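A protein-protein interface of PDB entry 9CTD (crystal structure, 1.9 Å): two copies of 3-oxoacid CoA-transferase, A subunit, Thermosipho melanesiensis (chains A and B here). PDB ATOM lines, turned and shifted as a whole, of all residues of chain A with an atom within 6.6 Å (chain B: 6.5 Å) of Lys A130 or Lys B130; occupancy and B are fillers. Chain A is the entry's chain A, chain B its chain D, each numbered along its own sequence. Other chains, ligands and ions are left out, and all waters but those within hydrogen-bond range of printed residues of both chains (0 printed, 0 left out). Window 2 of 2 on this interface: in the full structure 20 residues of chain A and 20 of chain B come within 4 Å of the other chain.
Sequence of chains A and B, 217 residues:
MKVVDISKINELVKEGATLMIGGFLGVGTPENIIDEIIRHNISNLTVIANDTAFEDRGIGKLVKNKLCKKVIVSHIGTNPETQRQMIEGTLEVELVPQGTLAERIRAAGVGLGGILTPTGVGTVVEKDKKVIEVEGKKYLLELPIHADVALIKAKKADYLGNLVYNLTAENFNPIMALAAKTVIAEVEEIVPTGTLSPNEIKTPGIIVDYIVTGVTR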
ATOM      1  N   GLU A 126      15.067  27.830 -18.394  1.00  0.00           N
ATOM      2  CA  GLU A 126      14.845  28.390 -19.723  1.00  0.00           C
ATOM      3  C   GLU A 126      15.893  27.921 -20.736  1.00  0.00           C
ATOM      4  O   GLU A 126      15.623  27.957 -21.941  1.00  0.00           O
ATOM      5  CB  GLU A 126      14.806  29.918 -19.640  1.00  0.00           C
ATOM      6  CG  GLU A 126      14.705  30.651 -20.967  1.00  0.00           C
ATOM      7  CD  GLU A 126      14.327  32.111 -20.821  1.00  0.00           C
ATOM      8  OE1 GLU A 126      13.729  32.483 -19.788  1.00  0.00           O
ATOM      9  OE2 GLU A 126      14.630  32.894 -21.748  1.00  0.00           O
ATOM     10  N   ASP A 128      17.759  26.271 -23.463  1.00  0.00           N
ATOM     11  CA  ASP A 128      17.401  25.316 -24.507  1.00  0.00           C
ATOM     12  C   ASP A 128      15.897  25.070 -24.571  1.00  0.00           C
ATOM     13  O   ASP A 128      15.459  23.967 -24.924  1.00  0.00           O
ATOM     14  CB  ASP A 128      18.122  23.977 -24.297  1.00  0.00           C
ATOM     15  CG  ASP A 128      19.626  24.092 -24.456  1.00  0.00           C
ATOM     16  OD1 ASP A 128      20.076  24.916 -25.271  1.00  0.00           O
ATOM     17  OD2 ASP A 128      20.347  23.396 -23.716  1.00  0.00           O
ATOM     18  N   LYS A 129      15.092  26.076 -24.243  1.00  0.00           N
ATOM     19  CA  LYS A 129      13.660  25.996 -24.475  1.00  0.00           C
ATOM     20  C   LYS A 129      13.249  27.063 -25.465  1.00  0.00           C
ATOM     21  O   LYS A 129      13.860  28.136 -25.544  1.00  0.00           O
ATOM     22  CB  LYS A 129      12.826  26.161 -23.178  1.00  0.00           C
ATOM     23  CG  LYS A 129      13.349  25.237 -22.152  1.00  0.00           C
ATOM     24  CD  LYS A 129      12.465  24.011 -22.039  1.00  0.00           C
ATOM     25  CE  LYS A 129      13.051  23.065 -21.045  1.00  0.00           C
ATOM     26  NZ  LYS A 129      12.707  23.502 -19.690  1.00  0.00           N
ATOM     27  N   LYS A 130      12.231  26.759 -26.251  1.00  0.00           N
ATOM     28  CA  LYS A 130      11.620  27.806 -27.040  1.00  0.00           C
ATOM     29  C   LYS A 130      10.827  28.681 -26.090  1.00  0.00           C
ATOM     30  O   LYS A 130      10.088  28.174 -25.242  1.00  0.00           O
ATOM     31  CB  LYS A 130      10.727  27.241 -28.142  1.00  0.00           C
ATOM     32  CG  LYS A 130      10.163  28.366 -29.033  1.00  0.00           C
ATOM     33  CD  LYS A 130       9.231  27.919 -30.161  1.00  0.00           C
ATOM     34  CE  LYS A 130       9.301  28.926 -31.337  1.00  0.00           C
ATOM     35  NZ  LYS A 130       8.208  28.749 -32.345  1.00  0.00           N
ATOM     36  N   VAL A 131      10.994  29.992 -26.215  1.00  0.00           N
ATOM     37  CA  VAL A 131      10.217  30.969 -25.471  1.00  0.00           C
ATOM     38  C   VAL A 131       9.147  31.509 -26.393  1.00  0.00           C
ATOM     39  O   VAL A 131       9.435  31.883 -27.534  1.00  0.00           O
ATOM     40  CB  VAL A 131      11.105  32.105 -24.937  1.00  0.00           C
ATOM     41  CG1 VAL A 131      10.282  33.095 -24.161  1.00  0.00           C
ATOM     42  CG2 VAL A 131      12.197  31.533 -24.087  1.00  0.00           C
ATOM     43  N   ILE A 132       7.913  31.543 -25.914  1.00  0.00           N
ATOM     44  CA  ILE A 132       6.786  32.056 -26.672  1.00  0.00           C
ATOM     45  C   ILE A 132       6.120  33.132 -25.853  1.00  0.00           C
ATOM     46  O   ILE A 132       5.782  32.906 -24.685  1.00  0.00           O
ATOM     47  CB  ILE A 132       5.791  30.936 -27.015  1.00  0.00           C
ATOM     48  CG1 ILE A 132       6.527  29.793 -27.721  1.00  0.00           C
ATOM     49  CG2 ILE A 132       4.682  31.475 -27.874  1.00  0.00           C
ATOM     50  CD1 ILE A 132       5.610  28.757 -28.344  1.00  0.00           C
ATOM     51  N   TYR A 139       6.440  32.653 -21.922  1.00  0.00           N
ATOM     52  CA  TYR A 139       6.219  31.273 -21.502  1.00  0.00           C
ATOM     53  C   TYR A 139       7.301  30.379 -22.077  1.00  0.00           C
ATOM     54  O   TYR A 139       7.827  30.630 -23.169  1.00  0.00           O
ATOM     55  CB  TYR A 139       4.849  30.735 -21.942  1.00  0.00           C
ATOM     56  CG  TYR A 139       3.705  31.549 -21.428  1.00  0.00           C
ATOM     57  CD1 TYR A 139       3.238  32.655 -22.139  1.00  0.00           C
ATOM     58  CD2 TYR A 139       3.106  31.240 -20.204  1.00  0.00           C
ATOM     59  CE1 TYR A 139       2.205  33.419 -21.654  1.00  0.00           C
ATOM     60  CE2 TYR A 139       2.066  32.015 -19.708  1.00  0.00           C
ATOM     61  CZ  TYR A 139       1.631  33.104 -20.459  1.00  0.00           C
ATOM     62  OH  TYR A 139       0.600  33.868 -20.011  1.00  0.00           O
ATOM     63  N   LEU A 140       7.631  29.329 -21.334  1.00  0.00           N
ATOM     64  CA  LEU A 140       8.469  28.270 -21.874  1.00  0.00           C
ATOM     65  C   LEU A 140       7.592  27.235 -22.575  1.00  0.00           C
ATOM     66  O   LEU A 140       6.594  26.787 -22.011  1.00  0.00           O
ATOM     67  CB  LEU A 140       9.272  27.584 -20.789  1.00  0.00           C
ATOM     68  CG  LEU A 140      10.120  28.522 -19.941  1.00  0.00           C
ATOM     69  CD1 LEU A 140      10.938  27.684 -19.004  1.00  0.00           C
ATOM     70  CD2 LEU A 140      11.023  29.370 -20.828  1.00  0.00           C
ATOM     71  N   LEU A 141       7.969  26.848 -23.792  1.00  0.00           N
ATOM     72  CA  LEU A 141       7.356  25.694 -24.445  1.00  0.00           C
ATOM     73  C   LEU A 141       7.972  24.437 -23.849  1.00  0.00           C
ATOM     74  O   LEU A 141       9.188  24.228 -23.941  1.00  0.00           O
ATOM     75  CB  LEU A 141       7.584  25.712 -25.950  1.00  0.00           C
ATOM     76  CG  LEU A 141       7.131  24.433 -26.664  1.00  0.00           C
ATOM     77  CD1 LEU A 141       5.641  24.235 -26.545  1.00  0.00           C
ATOM     78  CD2 LEU A 141       7.544  24.546 -28.120  1.00  0.00           C
ATOM     79  N   GLU A 142       7.141  23.590 -23.249  1.00  0.00           N
ATOM     80  CA  GLU A 142       7.610  22.352 -22.627  1.00  0.00           C
ATOM     81  C   GLU A 142       6.948  21.165 -23.324  1.00  0.00           C
ATOM     82  O   GLU A 142       5.760  21.212 -23.660  1.00  0.00           O
ATOM     83  CB  GLU A 142       7.309  22.360 -21.143  1.00  0.00           C
ATOM     84  CG  GLU A 142       8.042  23.465 -20.376  1.00  0.00           C
ATOM     85  CD  GLU A 142       9.444  23.111 -19.998  1.00  0.00           C
ATOM     86  OE1 GLU A 142       9.955  22.042 -20.426  1.00  0.00           O
ATOM     87  OE2 GLU A 142      10.062  23.925 -19.271  1.00  0.00           O
ATOM     88  N   GLU B 126      -7.236  25.993 -38.573  1.00  0.00           N
ATOM     89  CA  GLU B 126      -5.873  26.500 -38.620  1.00  0.00           C
ATOM     90  C   GLU B 126      -5.806  28.001 -38.932  1.00  0.00           C
ATOM     91  O   GLU B 126      -4.789  28.637 -38.634  1.00  0.00           O
ATOM     92  CB  GLU B 126      -5.053  25.713 -39.648  1.00  0.00           C
ATOM     93  CG  GLU B 126      -3.604  26.220 -39.810  1.00  0.00           C
ATOM     94  CD  GLU B 126      -2.728  25.269 -40.607  1.00  0.00           C
ATOM     95  OE1 GLU B 126      -3.054  24.070 -40.657  1.00  0.00           O
ATOM     96  OE2 GLU B 126      -1.702  25.708 -41.173  1.00  0.00           O
ATOM     97  N   ASP B 128      -5.540  31.726 -38.785  1.00  0.00           N
ATOM     98  CA  ASP B 128      -5.202  32.688 -37.749  1.00  0.00           C
ATOM     99  C   ASP B 128      -4.650  32.013 -36.497  1.00  0.00           C
ATOM    100  O   ASP B 128      -4.812  32.524 -35.384  1.00  0.00           O
ATOM    101  CB  ASP B 128      -6.419  33.544 -37.400  1.00  0.00           C
ATOM    102  CG  ASP B 128      -6.843  34.427 -38.553  1.00  0.00           C
ATOM    103  OD1 ASP B 128      -5.965  34.773 -39.376  1.00  0.00           O
ATOM    104  OD2 ASP B 128      -8.052  34.720 -38.664  1.00  0.00           O
ATOM    105  N   LYS B 129      -3.986  30.869 -36.656  1.00  0.00           N
ATOM    106  CA  LYS B 129      -3.315  30.221 -35.539  1.00  0.00           C
ATOM    107  C   LYS B 129      -1.837  30.135 -35.842  1.00  0.00           C
ATOM    108  O   LYS B 129      -1.440  29.977 -37.001  1.00  0.00           O
ATOM    109  CB  LYS B 129      -3.873  28.800 -35.236  1.00  0.00           C
ATOM    110  CG  LYS B 129      -5.327  28.955 -35.008  1.00  0.00           C
ATOM    111  CD  LYS B 129      -5.714  28.813 -33.580  1.00  0.00           C
ATOM    112  CE  LYS B 129      -7.213  28.839 -33.461  1.00  0.00           C
ATOM    113  NZ  LYS B 129      -7.775  27.593 -33.937  1.00  0.00           N
ATOM    114  N   LYS B 130      -1.023  30.282 -34.804  1.00  0.00           N
ATOM    115  CA  LYS B 130       0.378  29.927 -34.923  1.00  0.00           C
ATOM    116  C   LYS B 130       0.495  28.409 -35.026  1.00  0.00           C
ATOM    117  O   LYS B 130      -0.154  27.667 -34.275  1.00  0.00           O
ATOM    118  CB  LYS B 130       1.148  30.480 -33.737  1.00  0.00           C
ATOM    119  CG  LYS B 130       2.650  30.250 -33.818  1.00  0.00           C
ATOM    120  CD  LYS B 130       3.402  31.122 -32.804  1.00  0.00           C
ATOM    121  CE  LYS B 130       4.627  30.407 -32.259  1.00  0.00           C
ATOM    122  NZ  LYS B 130       5.854  30.733 -33.050  1.00  0.00           N
ATOM    123  N   VAL B 131       1.270  27.949 -36.008  1.00  0.00           N
ATOM    124  CA  VAL B 131       1.546  26.535 -36.219  1.00  0.00           C
ATOM    125  C   VAL B 131       2.942  26.263 -35.703  1.00  0.00           C
ATOM    126  O   VAL B 131       3.889  26.970 -36.064  1.00  0.00           O
ATOM    127  CB  VAL B 131       1.425  26.162 -37.707  1.00  0.00           C
ATOM    128  CG1 VAL B 131       1.805  24.709 -37.946  1.00  0.00           C
ATOM    129  CG2 VAL B 131       0.020  26.428 -38.192  1.00  0.00           C
ATOM    130  N   ILE B 132       3.080  25.252 -34.851  1.00  0.00           N
ATOM    131  CA  ILE B 132       4.367  24.896 -34.271  1.00  0.00           C
ATOM    132  C   ILE B 132       4.660  23.455 -34.621  1.00  0.00           C
ATOM    133  O   ILE B 132       3.789  22.589 -34.479  1.00  0.00           O
ATOM    134  CB  ILE B 132       4.391  25.110 -32.746  1.00  0.00           C
ATOM    135  CG1 ILE B 132       4.025  26.560 -32.428  1.00  0.00           C
ATOM    136  CG2 ILE B 132       5.773  24.738 -32.207  1.00  0.00           C
ATOM    137  CD1 ILE B 132       4.241  26.956 -30.987  1.00  0.00           C
ATOM    138  N   TYR B 139       1.368  21.224 -35.024  1.00  0.00           N
ATOM    139  CA  TYR B 139       0.363  21.476 -34.008  1.00  0.00           C
ATOM    140  C   TYR B 139      -0.130  22.899 -34.154  1.00  0.00           C
ATOM    141  O   TYR B 139       0.608  23.788 -34.580  1.00  0.00           O
ATOM    142  CB  TYR B 139       0.919  21.296 -32.600  1.00  0.00           C
ATOM    143  CG  TYR B 139       1.420  19.921 -32.379  1.00  0.00           C
ATOM    144  CD1 TYR B 139       0.572  18.917 -31.902  1.00  0.00           C
ATOM    145  CD2 TYR B 139       2.739  19.592 -32.661  1.00  0.00           C
ATOM    146  CE1 TYR B 139       1.032  17.626 -31.724  1.00  0.00           C
ATOM    147  CE2 TYR B 139       3.193  18.310 -32.500  1.00  0.00           C
ATOM    148  CZ  TYR B 139       2.351  17.341 -32.023  1.00  0.00           C
ATOM    149  OH  TYR B 139       2.863  16.079 -31.872  1.00  0.00           O
ATOM    150  N   LEU B 140      -1.377  23.113 -33.776  1.00  0.00           N
ATOM    151  CA  LEU B 140      -1.907  24.453 -33.609  1.00  0.00           C
ATOM    152  C   LEU B 140      -1.667  24.917 -32.181  1.00  0.00           C
ATOM    153  O   LEU B 140      -1.953  24.180 -31.232  1.00  0.00           O
ATOM    154  CB  LEU B 140      -3.399  24.474 -33.913  1.00  0.00           C
ATOM    155  CG  LEU B 140      -3.845  23.998 -35.284  1.00  0.00           C
ATOM    156  CD1 LEU B 140      -5.324  24.334 -35.401  1.00  0.00           C
ATOM    157  CD2 LEU B 140      -3.021  24.697 -36.370  1.00  0.00           C
ATOM    158  N   LEU B 141      -1.129  26.125 -32.029  1.00  0.00           N
ATOM    159  CA  LEU B 141      -1.075  26.780 -30.728  1.00  0.00           C
ATOM    160  C   LEU B 141      -2.464  27.321 -30.429  1.00  0.00           C
ATOM    161  O   LEU B 141      -3.014  28.110 -31.208  1.00  0.00           O
ATOM    162  CB  LEU B 141      -0.030  27.894 -30.722  1.00  0.00           C
ATOM    163  CG  LEU B 141      -0.056  28.777 -29.468  1.00  0.00           C
ATOM    164  CD1 LEU B 141       0.336  27.970 -28.212  1.00  0.00           C
ATOM    165  CD2 LEU B 141       0.867  29.969 -29.620  1.00  0.00           C
ATOM    166  N   GLU B 142      -3.061  26.848 -29.334  1.00  0.00           N
ATOM    167  CA  GLU B 142      -4.379  27.273 -28.913  1.00  0.00           C
ATOM    168  C   GLU B 142      -4.264  27.925 -27.545  1.00  0.00           C
ATOM    169  O   GLU B 142      -3.563  27.429 -26.673  1.00  0.00           O
ATOM    170  CB  GLU B 142      -5.337  26.080 -28.908  1.00  0.00           C
ATOM    171  CG  GLU B 142      -5.533  25.499 -30.318  1.00  0.00           C
ATOM    172  CD  GLU B 142      -6.591  26.226 -31.119  1.00  0.00           C
ATOM    173  OE1 GLU B 142      -7.047  27.306 -30.677  1.00  0.00           O
ATOM    174  OE2 GLU B 142      -6.963  25.706 -32.198  1.00  0.00           O
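The side-chain amino group (NZ) of Lys A130 sits close to the side-chain amino group (NZ) of Lys B130 (3.2 Å).
The backbone carbonyl oxygen (O) of Lys B130 is in hydrogen-bond range of the backbone NH (N) of Leu B141, 2.9 Å away.
The backbone carbonyl oxygen (O) of Ile B132 is in hydrogen-bond range of the backbone NH (N) of Tyr B139, 2.8 Å away.
O of Lys A130 is in hydrogen-bond range of N of Leu A141 (2.9 Å).
O of Ile A132 is in hydrogen-bond range of N of Tyr A139, 2.9 Å away.
Among the printed residues, merely in contact across the chains: Ile A132 with Ile B132 (3.5 Å).
Of chain B, only Lys B130 (3.2 Å) comes within 4 Å of Lys A130.
Of the printed residues of chain B, Ile A132 touches Ile B132 (3.5 Å).
Printed residues of chain A within 4 Å of Ile B132: Ile A132.
The nearest printed residue of chain A that does not touch Ile B132 is Leu A141 (4.5 Å).
Of the 10 printed residues of chain B, 2 touch a printed residue of chain A.
Hydrophobic or aromatic side chains of chain B within 4 Å of the printed part of chain A: Ile B132.
Of the 10 printed residues of chain A, 2 touch a printed residue of chain B.
Among the printed residues, no Asp or Glu carboxylate lies within 4 Å of a Lys or Arg side-chain nitrogen of the other chain.
Lys B130 touches its own counterpart, Lys A130.
Ile B132 touches its own counterpart, Ile A132.
Positions printed for both chains: 126, 128, 129, 130, 131, 132, 139, 140, 141 and 142.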
